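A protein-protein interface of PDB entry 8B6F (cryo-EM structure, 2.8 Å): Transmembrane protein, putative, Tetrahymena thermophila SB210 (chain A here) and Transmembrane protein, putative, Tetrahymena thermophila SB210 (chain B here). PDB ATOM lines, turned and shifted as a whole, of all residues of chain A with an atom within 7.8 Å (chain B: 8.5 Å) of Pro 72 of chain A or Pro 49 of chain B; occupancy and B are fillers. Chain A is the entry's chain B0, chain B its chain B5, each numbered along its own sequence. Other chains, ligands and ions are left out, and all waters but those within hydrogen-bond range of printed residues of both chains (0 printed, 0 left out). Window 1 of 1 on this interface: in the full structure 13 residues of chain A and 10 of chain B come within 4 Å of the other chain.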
ATOM      1  N   GLU A  64      17.275  -6.245  22.068  1.00  0.00           N
ATOM      2  CA  GLU A  64      16.989  -7.137  20.950  1.00  0.00           C
ATOM      3  C   GLU A  64      17.029  -8.593  21.393  1.00  0.00           C
ATOM      4  O   GLU A  64      16.170  -9.391  21.004  1.00  0.00           O
ATOM      5  CB  GLU A  64      17.982  -6.893  19.814  1.00  0.00           C
ATOM      6  CG  GLU A  64      17.895  -5.499  19.217  1.00  0.00           C
ATOM      7  CD  GLU A  64      18.820  -5.314  18.032  1.00  0.00           C
ATOM      8  OE1 GLU A  64      19.561  -6.261  17.701  1.00  0.00           O
ATOM      9  OE2 GLU A  64      18.805  -4.220  17.428  1.00  0.00           O
ATOM     10  N   LYS A  65      18.028  -8.962  22.197  1.00  0.00           N
ATOM     11  CA  LYS A  65      18.092 -10.328  22.703  1.00  0.00           C
ATOM     12  C   LYS A  65      16.856 -10.658  23.527  1.00  0.00           C
ATOM     13  O   LYS A  65      16.271 -11.737  23.378  1.00  0.00           O
ATOM     14  CB  LYS A  65      19.358 -10.519  23.539  1.00  0.00           C
ATOM     15  CG  LYS A  65      20.646 -10.454  22.737  1.00  0.00           C
ATOM     16  CD  LYS A  65      21.865 -10.484  23.643  1.00  0.00           C
ATOM     17  CE  LYS A  65      23.149 -10.377  22.838  1.00  0.00           C
ATOM     18  NZ  LYS A  65      24.358 -10.371  23.710  1.00  0.00           N
ATOM     19  N   LEU A  66      16.445  -9.743  24.405  1.00  0.00           N
ATOM     20  CA  LEU A  66      15.282 -10.001  25.247  1.00  0.00           C
ATOM     21  C   LEU A  66      14.017 -10.166  24.416  1.00  0.00           C
ATOM     22  O   LEU A  66      13.199 -11.051  24.687  1.00  0.00           O
ATOM     23  CB  LEU A  66      15.112  -8.874  26.265  1.00  0.00           C
ATOM     24  CG  LEU A  66      16.211  -8.744  27.325  1.00  0.00           C
ATOM     25  CD1 LEU A  66      15.960  -7.535  28.200  1.00  0.00           C
ATOM     26  CD2 LEU A  66      16.310  -9.996  28.178  1.00  0.00           C
ATOM     27  N   ARG A  67      13.834  -9.322  23.398  1.00  0.00           N
ATOM     28  CA  ARG A  67      12.604  -9.370  22.617  1.00  0.00           C
ATOM     29  C   ARG A  67      12.565 -10.568  21.678  1.00  0.00           C
ATOM     30  O   ARG A  67      11.481 -11.090  21.393  1.00  0.00           O
ATOM     31  CB  ARG A  67      12.435  -8.076  21.820  1.00  0.00           C
ATOM     32  CG  ARG A  67      11.828  -6.933  22.618  1.00  0.00           C
ATOM     33  CD  ARG A  67      11.494  -5.746  21.725  1.00  0.00           C
ATOM     34  NE  ARG A  67      12.690  -5.111  21.183  1.00  0.00           N
ATOM     35  CZ  ARG A  67      13.346  -4.118  21.767  1.00  0.00           C
ATOM     36  NH1 ARG A  67      12.951  -3.612  22.923  1.00  0.00           N
ATOM     37  NH2 ARG A  67      14.429  -3.621  21.178  1.00  0.00           N
ATOM     38  N   HIS A  68      13.716 -11.021  21.184  1.00  0.00           N
ATOM     39  CA  HIS A  68      13.736 -12.065  20.169  1.00  0.00           C
ATOM     40  C   HIS A  68      13.954 -13.463  20.724  1.00  0.00           C
ATOM     41  O   HIS A  68      13.414 -14.423  20.166  1.00  0.00           O
ATOM     42  CB  HIS A  68      14.825 -11.775  19.131  1.00  0.00           C
ATOM     43  CG  HIS A  68      14.585 -12.432  17.808  1.00  0.00           C
ATOM     44  ND1 HIS A  68      13.533 -12.088  16.988  1.00  0.00           N
ATOM     45  CD2 HIS A  68      15.259 -13.413  17.161  1.00  0.00           C
ATOM     46  CE1 HIS A  68      13.567 -12.828  15.894  1.00  0.00           C
ATOM     47  NE2 HIS A  68      14.606 -13.640  15.975  1.00  0.00           N
ATOM     48  N   TYR A  69      14.727 -13.614  21.797  1.00  0.00           N
ATOM     49  CA  TYR A  69      15.082 -14.936  22.297  1.00  0.00           C
ATOM     50  C   TYR A  69      14.542 -15.210  23.689  1.00  0.00           C
ATOM     51  O   TYR A  69      13.948 -16.270  23.918  1.00  0.00           O
ATOM     52  CB  TYR A  69      16.611 -15.106  22.286  1.00  0.00           C
ATOM     53  CG  TYR A  69      17.182 -15.286  20.900  1.00  0.00           C
ATOM     54  CD1 TYR A  69      17.305 -16.550  20.341  1.00  0.00           C
ATOM     55  CD2 TYR A  69      17.586 -14.193  20.146  1.00  0.00           C
ATOM     56  CE1 TYR A  69      17.820 -16.722  19.074  1.00  0.00           C
ATOM     57  CE2 TYR A  69      18.103 -14.355  18.878  1.00  0.00           C
ATOM     58  CZ  TYR A  69      18.216 -15.623  18.347  1.00  0.00           C
ATOM     59  OH  TYR A  69      18.730 -15.793  17.083  1.00  0.00           O
ATOM     60  N   PHE A  70      14.733 -14.288  24.632  1.00  0.00           N
ATOM     61  CA  PHE A  70      14.344 -14.557  26.013  1.00  0.00           C
ATOM     62  C   PHE A  70      12.848 -14.817  26.130  1.00  0.00           C
ATOM     63  O   PHE A  70      12.423 -15.800  26.749  1.00  0.00           O
ATOM     64  CB  PHE A  70      14.756 -13.388  26.906  1.00  0.00           C
ATOM     65  CG  PHE A  70      14.085 -13.386  28.246  1.00  0.00           C
ATOM     66  CD1 PHE A  70      14.560 -14.174  29.277  1.00  0.00           C
ATOM     67  CD2 PHE A  70      12.981 -12.582  28.475  1.00  0.00           C
ATOM     68  CE1 PHE A  70      13.941 -14.166  30.512  1.00  0.00           C
ATOM     69  CE2 PHE A  70      12.360 -12.570  29.707  1.00  0.00           C
ATOM     70  CZ  PHE A  70      12.840 -13.363  30.726  1.00  0.00           C
ATOM     71  N   LYS A  71      12.028 -13.951  25.536  1.00  0.00           N
ATOM     72  CA  LYS A  71      10.582 -14.099  25.682  1.00  0.00           C
ATOM     73  C   LYS A  71      10.066 -15.383  25.053  1.00  0.00           C
ATOM     74  O   LYS A  71       9.313 -16.112  25.721  1.00  0.00           O
ATOM     75  CB  LYS A  71       9.878 -12.869  25.106  1.00  0.00           C
ATOM     76  CG  LYS A  71       9.738 -11.722  26.097  1.00  0.00           C
ATOM     77  CD  LYS A  71       8.764 -12.061  27.218  1.00  0.00           C
ATOM     78  CE  LYS A  71       8.559 -10.875  28.143  1.00  0.00           C
ATOM     79  NZ  LYS A  71       7.628 -11.194  29.259  1.00  0.00           N
ATOM     80  N   PRO A  72      10.405 -15.723  23.809  1.00  0.00           N
ATOM     81  CA  PRO A  72      10.000 -17.043  23.298  1.00  0.00           C
ATOM     82  C   PRO A  72      10.537 -18.189  24.133  1.00  0.00           C
ATOM     83  O   PRO A  72       9.845 -19.196  24.320  1.00  0.00           O
ATOM     84  CB  PRO A  72      10.566 -17.051  21.871  1.00  0.00           C
ATOM     85  CG  PRO A  72      10.657 -15.621  21.494  1.00  0.00           C
ATOM     86  CD  PRO A  72      11.003 -14.885  22.756  1.00  0.00           C
ATOM     87  N   ALA A  73      11.767 -18.065  24.635  1.00  0.00           N
ATOM     88  CA  ALA A  73      12.345 -19.138  25.436  1.00  0.00           C
ATOM     89  C   ALA A  73      11.550 -19.360  26.716  1.00  0.00           C
ATOM     90  O   ALA A  73      11.319 -20.505  27.121  1.00  0.00           O
ATOM     91  CB  ALA A  73      13.803 -18.818  25.762  1.00  0.00           C
ATOM     92  N   ILE A  74      11.124 -18.278  27.367  1.00  0.00           N
ATOM     93  CA  ILE A  74      10.437 -18.393  28.649  1.00  0.00           C
ATOM     94  C   ILE A  74       8.940 -18.638  28.500  1.00  0.00           C
ATOM     95  O   ILE A  74       8.302 -19.105  29.453  1.00  0.00           O
ATOM     96  CB  ILE A  74      10.690 -17.134  29.504  1.00  0.00           C
ATOM     97  CG1 ILE A  74      10.365 -17.398  30.976  1.00  0.00           C
ATOM     98  CG2 ILE A  74       9.873 -15.953  29.000  1.00  0.00           C
ATOM     99  CD1 ILE A  74      11.263 -18.411  31.649  1.00  0.00           C
ATOM    100  N   GLU A  75       8.362 -18.337  27.340  1.00  0.00           N
ATOM    101  CA  GLU A  75       6.972 -18.654  27.049  1.00  0.00           C
ATOM    102  C   GLU A  75       6.833 -19.897  26.183  1.00  0.00           C
ATOM    103  O   GLU A  75       5.738 -20.178  25.687  1.00  0.00           O
ATOM    104  CB  GLU A  75       6.294 -17.467  26.362  1.00  0.00           C
ATOM    105  CG  GLU A  75       6.406 -16.148  27.116  1.00  0.00           C
ATOM    106  CD  GLU A  75       5.728 -16.180  28.473  1.00  0.00           C
ATOM    107  OE1 GLU A  75       6.076 -17.048  29.300  1.00  0.00           O
ATOM    108  OE2 GLU A  75       4.843 -15.333  28.714  1.00  0.00           O
ATOM    109  N   TRP A  76       7.919 -20.642  25.988  1.00  0.00           N
ATOM    110  CA  TRP A  76       7.885 -21.814  25.129  1.00  0.00           C
ATOM    111  C   TRP A  76       6.890 -22.845  25.641  1.00  0.00           C
ATOM    112  O   TRP A  76       6.767 -23.072  26.848  1.00  0.00           O
ATOM    113  CB  TRP A  76       9.276 -22.437  25.043  1.00  0.00           C
ATOM    114  CG  TRP A  76       9.325 -23.693  24.234  1.00  0.00           C
ATOM    115  CD1 TRP A  76       9.326 -23.793  22.876  1.00  0.00           C
ATOM    116  CD2 TRP A  76       9.386 -25.033  24.736  1.00  0.00           C
ATOM    117  NE1 TRP A  76       9.383 -25.112  22.499  1.00  0.00           N
ATOM    118  CE2 TRP A  76       9.420 -25.894  23.623  1.00  0.00           C
ATOM    119  CE3 TRP A  76       9.413 -25.588  26.019  1.00  0.00           C
ATOM    120  CZ2 TRP A  76       9.480 -27.279  23.753  1.00  0.00           C
ATOM    121  CZ3 TRP A  76       9.473 -26.963  26.147  1.00  0.00           C
ATOM    122  CH2 TRP A  76       9.505 -27.794  25.019  1.00  0.00           C
ATOM    123  N   GLN A  77       6.181 -23.470  24.709  1.00  0.00           N
ATOM    124  CA  GLN A  77       5.326 -24.613  24.974  1.00  0.00           C
ATOM    125  C   GLN A  77       5.662 -25.718  23.986  1.00  0.00           C
ATOM    126  O   GLN A  77       6.126 -25.439  22.876  1.00  0.00           O
ATOM    127  CB  GLN A  77       3.840 -24.249  24.850  1.00  0.00           C
ATOM    128  CG  GLN A  77       3.379 -23.168  25.811  1.00  0.00           C
ATOM    129  CD  GLN A  77       3.376 -23.632  27.251  1.00  0.00           C
ATOM    130  OE1 GLN A  77       3.753 -24.761  27.552  1.00  0.00           O
ATOM    131  NE2 GLN A  77       2.943 -22.758  28.151  1.00  0.00           N
ATOM    132  N   TYR A  80       4.103 -25.063  20.602  1.00  0.00           N
ATOM    133  CA  TYR A  80       4.351 -23.813  19.890  1.00  0.00           C
ATOM    134  C   TYR A  80       5.242 -24.006  18.672  1.00  0.00           C
ATOM    135  O   TYR A  80       5.065 -23.310  17.668  1.00  0.00           O
ATOM    136  CB  TYR A  80       4.979 -22.771  20.818  1.00  0.00           C
ATOM    137  CG  TYR A  80       4.010 -22.119  21.774  1.00  0.00           C
ATOM    138  CD1 TYR A  80       2.664 -22.454  21.768  1.00  0.00           C
ATOM    139  CD2 TYR A  80       4.433 -21.128  22.648  1.00  0.00           C
ATOM    140  CE1 TYR A  80       1.777 -21.852  22.618  1.00  0.00           C
ATOM    141  CE2 TYR A  80       3.547 -20.515  23.509  1.00  0.00           C
ATOM    142  CZ  TYR A  80       2.215 -20.878  23.475  1.00  0.00           C
ATOM    143  OH  TYR A  80       1.297 -20.298  24.310  1.00  0.00           O
ATOM    144  N   THR A  88      13.357 -20.413  14.301  1.00  0.00           N
ATOM    145  CA  THR A  88      14.419 -19.418  14.281  1.00  0.00           C
ATOM    146  C   THR A  88      15.767 -20.092  14.493  1.00  0.00           C
ATOM    147  O   THR A  88      15.881 -21.074  15.231  1.00  0.00           O
ATOM    148  CB  THR A  88      14.184 -18.362  15.362  1.00  0.00           C
ATOM    149  OG1 THR A  88      14.201 -18.979  16.655  1.00  0.00           O
ATOM    150  CG2 THR A  88      12.844 -17.671  15.152  1.00  0.00           C
ATOM    151  N   LYS B  43       1.212 -20.835  13.180  1.00  0.00           N
ATOM    152  CA  LYS B  43       1.948 -20.930  14.435  1.00  0.00           C
ATOM    153  C   LYS B  43       2.879 -19.742  14.632  1.00  0.00           C
ATOM    154  O   LYS B  43       3.124 -19.332  15.771  1.00  0.00           O
ATOM    155  CB  LYS B  43       2.734 -22.239  14.488  1.00  0.00           C
ATOM    156  CG  LYS B  43       1.862 -23.461  14.728  1.00  0.00           C
ATOM    157  CD  LYS B  43       2.696 -24.724  14.824  1.00  0.00           C
ATOM    158  CE  LYS B  43       1.845 -25.922  15.202  1.00  0.00           C
ATOM    159  NZ  LYS B  43       2.648 -27.173  15.283  1.00  0.00           N
ATOM    160  N   LYS B  44       3.408 -19.182  13.544  1.00  0.00           N
ATOM    161  CA  LYS B  44       4.251 -18.000  13.652  1.00  0.00           C
ATOM    162  C   LYS B  44       3.446 -16.735  13.902  1.00  0.00           C
ATOM    163  O   LYS B  44       4.008 -15.746  14.384  1.00  0.00           O
ATOM    164  CB  LYS B  44       5.086 -17.830  12.381  1.00  0.00           C
ATOM    165  CG  LYS B  44       6.116 -16.709  12.459  1.00  0.00           C
ATOM    166  CD  LYS B  44       6.960 -16.638  11.193  1.00  0.00           C
ATOM    167  CE  LYS B  44       8.010 -15.541  11.295  1.00  0.00           C
ATOM    168  NZ  LYS B  44       8.804 -15.400  10.042  1.00  0.00           N
ATOM    169  N   LEU B  45       2.150 -16.741  13.592  1.00  0.00           N
ATOM    170  CA  LEU B  45       1.332 -15.541  13.684  1.00  0.00           C
ATOM    171  C   LEU B  45       0.444 -15.497  14.919  1.00  0.00           C
ATOM    172  O   LEU B  45       0.109 -14.401  15.379  1.00  0.00           O
ATOM    173  CB  LEU B  45       0.459 -15.412  12.431  1.00  0.00           C
ATOM    174  CG  LEU B  45      -0.381 -14.142  12.288  1.00  0.00           C
ATOM    175  CD1 LEU B  45       0.499 -12.905  12.231  1.00  0.00           C
ATOM    176  CD2 LEU B  45      -1.249 -14.233  11.048  1.00  0.00           C
ATOM    177  N   TYR B  46       0.051 -16.648  15.470  1.00  0.00           N
ATOM    178  CA  TYR B  46      -0.878 -16.687  16.592  1.00  0.00           C
ATOM    179  C   TYR B  46      -0.345 -17.396  17.828  1.00  0.00           C
ATOM    180  O   TYR B  46      -0.957 -17.273  18.894  1.00  0.00           O
ATOM    181  CB  TYR B  46      -2.195 -17.361  16.175  1.00  0.00           C
ATOM    182  CG  TYR B  46      -2.911 -16.643  15.059  1.00  0.00           C
ATOM    183  CD1 TYR B  46      -3.430 -15.371  15.248  1.00  0.00           C
ATOM    184  CD2 TYR B  46      -3.080 -17.242  13.820  1.00  0.00           C
ATOM    185  CE1 TYR B  46      -4.088 -14.712  14.232  1.00  0.00           C
ATOM    186  CE2 TYR B  46      -3.735 -16.593  12.797  1.00  0.00           C
ATOM    187  CZ  TYR B  46      -4.237 -15.328  13.009  1.00  0.00           C
ATOM    188  OH  TYR B  46      -4.895 -14.678  11.991  1.00  0.00           O
ATOM    189  N   LEU B  47       0.755 -18.132  17.724  1.00  0.00           N
ATOM    190  CA  LEU B  47       1.361 -18.821  18.856  1.00  0.00           C
ATOM    191  C   LEU B  47       2.779 -18.322  19.092  1.00  0.00           C
ATOM    192  O   LEU B  47       3.705 -19.101  19.323  1.00  0.00           O
ATOM    193  CB  LEU B  47       1.353 -20.333  18.642  1.00  0.00           C
ATOM    194  CG  LEU B  47      -0.019 -21.006  18.547  1.00  0.00           C
ATOM    195  CD1 LEU B  47       0.147 -22.504  18.383  1.00  0.00           C
ATOM    196  CD2 LEU B  47      -0.882 -20.697  19.761  1.00  0.00           C
ATOM    197  N   ASN B  48       2.960 -17.008  19.031  1.00  0.00           N
ATOM    198  CA  ASN B  48       4.253 -16.378  19.222  1.00  0.00           C
ATOM    199  C   ASN B  48       4.097 -15.182  20.149  1.00  0.00           C
ATOM    200  O   ASN B  48       3.051 -14.526  20.142  1.00  0.00           O
ATOM    201  CB  ASN B  48       4.838 -15.923  17.875  1.00  0.00           C
ATOM    202  CG  ASN B  48       6.273 -15.460  17.986  1.00  0.00           C
ATOM    203  OD1 ASN B  48       6.542 -14.284  18.228  1.00  0.00           O
ATOM    204  ND2 ASN B  48       7.209 -16.384  17.803  1.00  0.00           N
ATOM    205  N   PRO B  49       5.112 -14.877  20.963  1.00  0.00           N
ATOM    206  CA  PRO B  49       5.022 -13.666  21.796  1.00  0.00           C
ATOM    207  C   PRO B  49       4.835 -12.399  20.983  1.00  0.00           C
ATOM    208  O   PRO B  49       4.177 -11.462  21.450  1.00  0.00           O
ATOM    209  CB  PRO B  49       6.356 -13.664  22.556  1.00  0.00           C
ATOM    210  CG  PRO B  49       6.784 -15.082  22.570  1.00  0.00           C
ATOM    211  CD  PRO B  49       6.316 -15.666  21.273  1.00  0.00           C
ATOM    212  N   ARG B  50       5.400 -12.342  19.777  1.00  0.00           N
ATOM    213  CA  ARG B  50       5.218 -11.214  18.867  1.00  0.00           C
ATOM    214  C   ARG B  50       5.739  -9.909  19.462  1.00  0.00           C
ATOM    215  O   ARG B  50       5.221  -8.830  19.168  1.00  0.00           O
ATOM    216  CB  ARG B  50       3.748 -11.067  18.463  1.00  0.00           C
ATOM    217  CG  ARG B  50       3.237 -12.232  17.628  1.00  0.00           C
ATOM    218  CD  ARG B  50       1.766 -12.082  17.281  1.00  0.00           C
ATOM    219  NE  ARG B  50       1.502 -10.896  16.475  1.00  0.00           N
ATOM    220  CZ  ARG B  50       0.338 -10.624  15.902  1.00  0.00           C
ATOM    221  NH1 ARG B  50      -0.694 -11.444  16.010  1.00  0.00           N
ATOM    222  NH2 ARG B  50       0.205  -9.503  15.200  1.00  0.00           N
ATOM    223  N   TYR B  51       6.769  -9.995  20.303  1.00  0.00           N
ATOM    224  CA  TYR B  51       7.459  -8.803  20.773  1.00  0.00           C
ATOM    225  C   TYR B  51       8.482  -8.285  19.773  1.00  0.00           C
ATOM    226  O   TYR B  51       8.982  -7.168  19.944  1.00  0.00           O
ATOM    227  CB  TYR B  51       8.156  -9.086  22.106  1.00  0.00           C
ATOM    228  CG  TYR B  51       7.208  -9.296  23.260  1.00  0.00           C
ATOM    229  CD1 TYR B  51       6.351  -8.285  23.674  1.00  0.00           C
ATOM    230  CD2 TYR B  51       7.184 -10.500  23.950  1.00  0.00           C
ATOM    231  CE1 TYR B  51       5.487  -8.472  24.734  1.00  0.00           C
ATOM    232  CE2 TYR B  51       6.323 -10.696  25.012  1.00  0.00           C
ATOM    233  CZ  TYR B  51       5.478  -9.679  25.398  1.00  0.00           C
ATOM    234  OH  TYR B  51       4.621  -9.872  26.456  1.00  0.00           O
ATOM    235  N   SER B  52       8.799  -9.061  18.741  1.00  0.00           N
ATOM    236  CA  SER B  52       9.742  -8.671  17.705  1.00  0.00           C
ATOM    237  C   SER B  52       9.011  -8.546  16.376  1.00  0.00           C
ATOM    238  O   SER B  52       8.191  -9.399  16.024  1.00  0.00           O
ATOM    239  CB  SER B  52      10.877  -9.691  17.583  1.00  0.00           C
ATOM    240  OG  SER B  52      11.803  -9.298  16.583  1.00  0.00           O
ATOM    241  N   THR B  54       8.418  -9.250  13.106  1.00  0.00           N
ATOM    242  CA  THR B  54       8.820 -10.288  12.166  1.00  0.00           C
ATOM    243  C   THR B  54       7.933 -10.375  10.936  1.00  0.00           C
ATOM    244  O   THR B  54       8.431 -10.710   9.859  1.00  0.00           O
ATOM    245  CB  THR B  54       8.833 -11.657  12.856  1.00  0.00           C
ATOM    246  OG1 THR B  54       9.563 -11.572  14.087  1.00  0.00           O
ATOM    247  CG2 THR B  54       9.488 -12.699  11.963  1.00  0.00           C
ATOM    248  N   MET B  55       6.638 -10.088  11.062  1.00  0.00           N
ATOM    249  CA  MET B  55       5.721 -10.136   9.927  1.00  0.00           C
ATOM    250  C   MET B  55       5.235  -8.728   9.610  1.00  0.00           C
ATOM    251  O   MET B  55       4.339  -8.213  10.296  1.00  0.00           O
ATOM    252  CB  MET B  55       4.533 -11.054  10.229  1.00  0.00           C
ATOM    253  CG  MET B  55       4.907 -12.515  10.413  1.00  0.00           C
ATOM    254  SD  MET B  55       5.429 -12.918  12.088  1.00  0.00           S
ATOM    255  CE  MET B  55       3.868 -12.824  12.952  1.00  0.00           C
ATOM    256  N   GLN B  59       1.916  -7.142  12.089  1.00  0.00           N
ATOM    257  CA  GLN B  59       2.200  -6.590  13.403  1.00  0.00           C
ATOM    258  C   GLN B  59       2.222  -5.070  13.323  1.00  0.00           C
ATOM    259  O   GLN B  59       2.625  -4.487  12.313  1.00  0.00           O
ATOM    260  CB  GLN B  59       3.542  -7.099  13.933  1.00  0.00           C
ATOM    261  CG  GLN B  59       3.626  -8.607  14.080  1.00  0.00           C
ATOM    262  CD  GLN B  59       4.865  -9.042  14.833  1.00  0.00           C
ATOM    263  OE1 GLN B  59       5.593  -8.220  15.384  1.00  0.00           O
ATOM    264  NE2 GLN B  59       5.111 -10.346  14.863  1.00  0.00           N
ATOM    265  N   TYR B  68       8.705  -4.379  26.664  1.00  0.00           N
ATOM    266  CA  TYR B  68       7.832  -5.407  26.106  1.00  0.00           C
ATOM    267  C   TYR B  68       6.495  -4.774  25.749  1.00  0.00           C
ATOM    268  O   TYR B  68       5.716  -4.414  26.639  1.00  0.00           O
ATOM    269  CB  TYR B  68       7.636  -6.556  27.094  1.00  0.00           C
ATOM    270  CG  TYR B  68       8.921  -7.213  27.536  1.00  0.00           C
ATOM    271  CD1 TYR B  68       9.675  -7.973  26.653  1.00  0.00           C
ATOM    272  CD2 TYR B  68       9.369  -7.087  28.841  1.00  0.00           C
ATOM    273  CE1 TYR B  68      10.847  -8.580  27.057  1.00  0.00           C
ATOM    274  CE2 TYR B  68      10.539  -7.689  29.257  1.00  0.00           C
ATOM    275  CZ  TYR B  68      11.273  -8.435  28.361  1.00  0.00           C
ATOM    276  OH  TYR B  68      12.438  -9.035  28.771  1.00  0.00           O
ATOM    277  N   GLU B  69       6.232  -4.637  24.452  1.00  0.00           N
ATOM    278  CA  GLU B  69       4.928  -4.216  23.957  1.00  0.00           C
ATOM    279  C   GLU B  69       4.582  -5.080  22.757  1.00  0.00           C
ATOM    280  O   GLU B  69       5.359  -5.153  21.801  1.00  0.00           O
ATOM    281  CB  GLU B  69       4.923  -2.733  23.573  1.00  0.00           C
ATOM    282  CG  GLU B  69       5.161  -1.792  24.743  1.00  0.00           C
ATOM    283  CD  GLU B  69       4.896  -0.341  24.389  1.00  0.00           C
ATOM    284  OE1 GLU B  69       4.392  -0.083  23.276  1.00  0.00           O
ATOM    285  OE2 GLU B  69       5.188   0.540  25.223  1.00  0.00           O
ATOM    286  N   LYS B  70       3.425  -5.733  22.806  1.00  0.00           N
ATOM    287  CA  LYS B  70       3.025  -6.622  21.725  1.00  0.00           C
ATOM    288  C   LYS B  70       2.774  -5.823  20.453  1.00  0.00           C
ATOM    289  O   LYS B  70       2.057  -4.818  20.469  1.00  0.00           O
ATOM    290  CB  LYS B  70       1.774  -7.404  22.119  1.00  0.00           C
ATOM    291  CG  LYS B  70       1.338  -8.431  21.085  1.00  0.00           C
ATOM    292  CD  LYS B  70       0.111  -9.196  21.549  1.00  0.00           C
ATOM    293  CE  LYS B  70      -0.332 -10.210  20.506  1.00  0.00           C
ATOM    294  NZ  LYS B  70      -1.522 -10.987  20.958  1.00  0.00           N
ATOM    295  N   LEU B  71       3.361  -6.276  19.349  1.00  0.00           N
ATOM    296  CA  LEU B  71       3.217  -5.596  18.068  1.00  0.00           C
ATOM    297  C   LEU B  71       2.179  -6.294  17.199  1.00  0.00           C
ATOM    298  O   LEU B  71       1.924  -7.486  17.360  1.00  0.00           O
ATOM    299  CB  LEU B  71       4.561  -5.539  17.338  1.00  0.00           C
ATOM    300  CG  LEU B  71       5.703  -4.838  18.080  1.00  0.00           C
ATOM    301  CD1 LEU B  71       6.988  -4.922  17.276  1.00  0.00           C
ATOM    302  CD2 LEU B  71       5.357  -3.390  18.381  1.00  0.00           C
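Among the printed residues, pairs that only touch across the chains: Leu 66 of chain A with Tyr 68 of chain B (3.7 Å), Arg 67 of chain A with Tyr 51 of chain B (3.4 Å), Phe 70 of chain A with Tyr 68 of chain B (3.6 Å), Lys 71 of chain A with Tyr 51 of chain B (3.6 Å), Lys 71 of chain A with Tyr 68 of chain B (3.4 Å), Pro 72 of chain A with Pro 49 of chain B (3.8 Å), Tyr 80 of chain A with Lys 43 of chain B (3.96 Å) and Tyr 80 of chain A with Leu 47 of chain B (3.9 Å).
O of Ser 52 of chain B lies within hydrogen-bond range of OG1 of Thr 54 of chain B.
N of Phe 70 of chain A is in hydrogen-bond range of O of Lys 65 of chain A (3.2 Å).
The backbone carbonyl oxygen (O) of Ser 52 of chain B sits close to the side-chain amide oxygen (OE1) of Gln 59 of chain B (2.9 Å).
The backbone carbonyl oxygen (O) of Leu 66 of chain A is in hydrogen-bond range of the backbone NH (N) of Lys 71 of chain A (3.2 Å).
ND1 of His 68 of chain A sits at hydrogen-bond distance from OG of Ser 52 of chain B (3.3 Å).
Hydrophobic or aromatic side chains of chain B within 4 Å of the printed part of chain A: Leu 47, Pro 49, Tyr 51 and Tyr 68.
Of the 16 printed residues of chain A, 7 touch a printed residue of chain B.
Hydrophobic or aromatic side chains of chain A that line the printed part of chain B: Leu 66, His 68, Phe 70 and Tyr 80.
Among the printed residues, 9 pairs touch across the chains.
Printed residues of chain B within 4 Å of Leu 66 of chain A: Tyr 68 (3.7 Å).
Printed residues of chain B within 4 Å of His 68 of chain A: Ser 52 (3.3 Å).
Printed residues of chain B within 4 Å of Pro 72 of chain A: Pro 49 (3.8 Å).
No residue of chain B comes within 4 Å of Ala 73 of chain A.
Leu 45 of chain B touches none of the printed residues of chain A.
No residue of chain A comes within 4 Å of Asn 48 of chain B.
Of chain A, only Pro 72 comes within 4 Å of Pro 49 of chain B.
Glu 69 of chain B touches none of the printed residues of chain A.
The nearest residue of chain A that does not touch Pro 49 of chain B is Lys 71 of chain A (4.1 Å).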
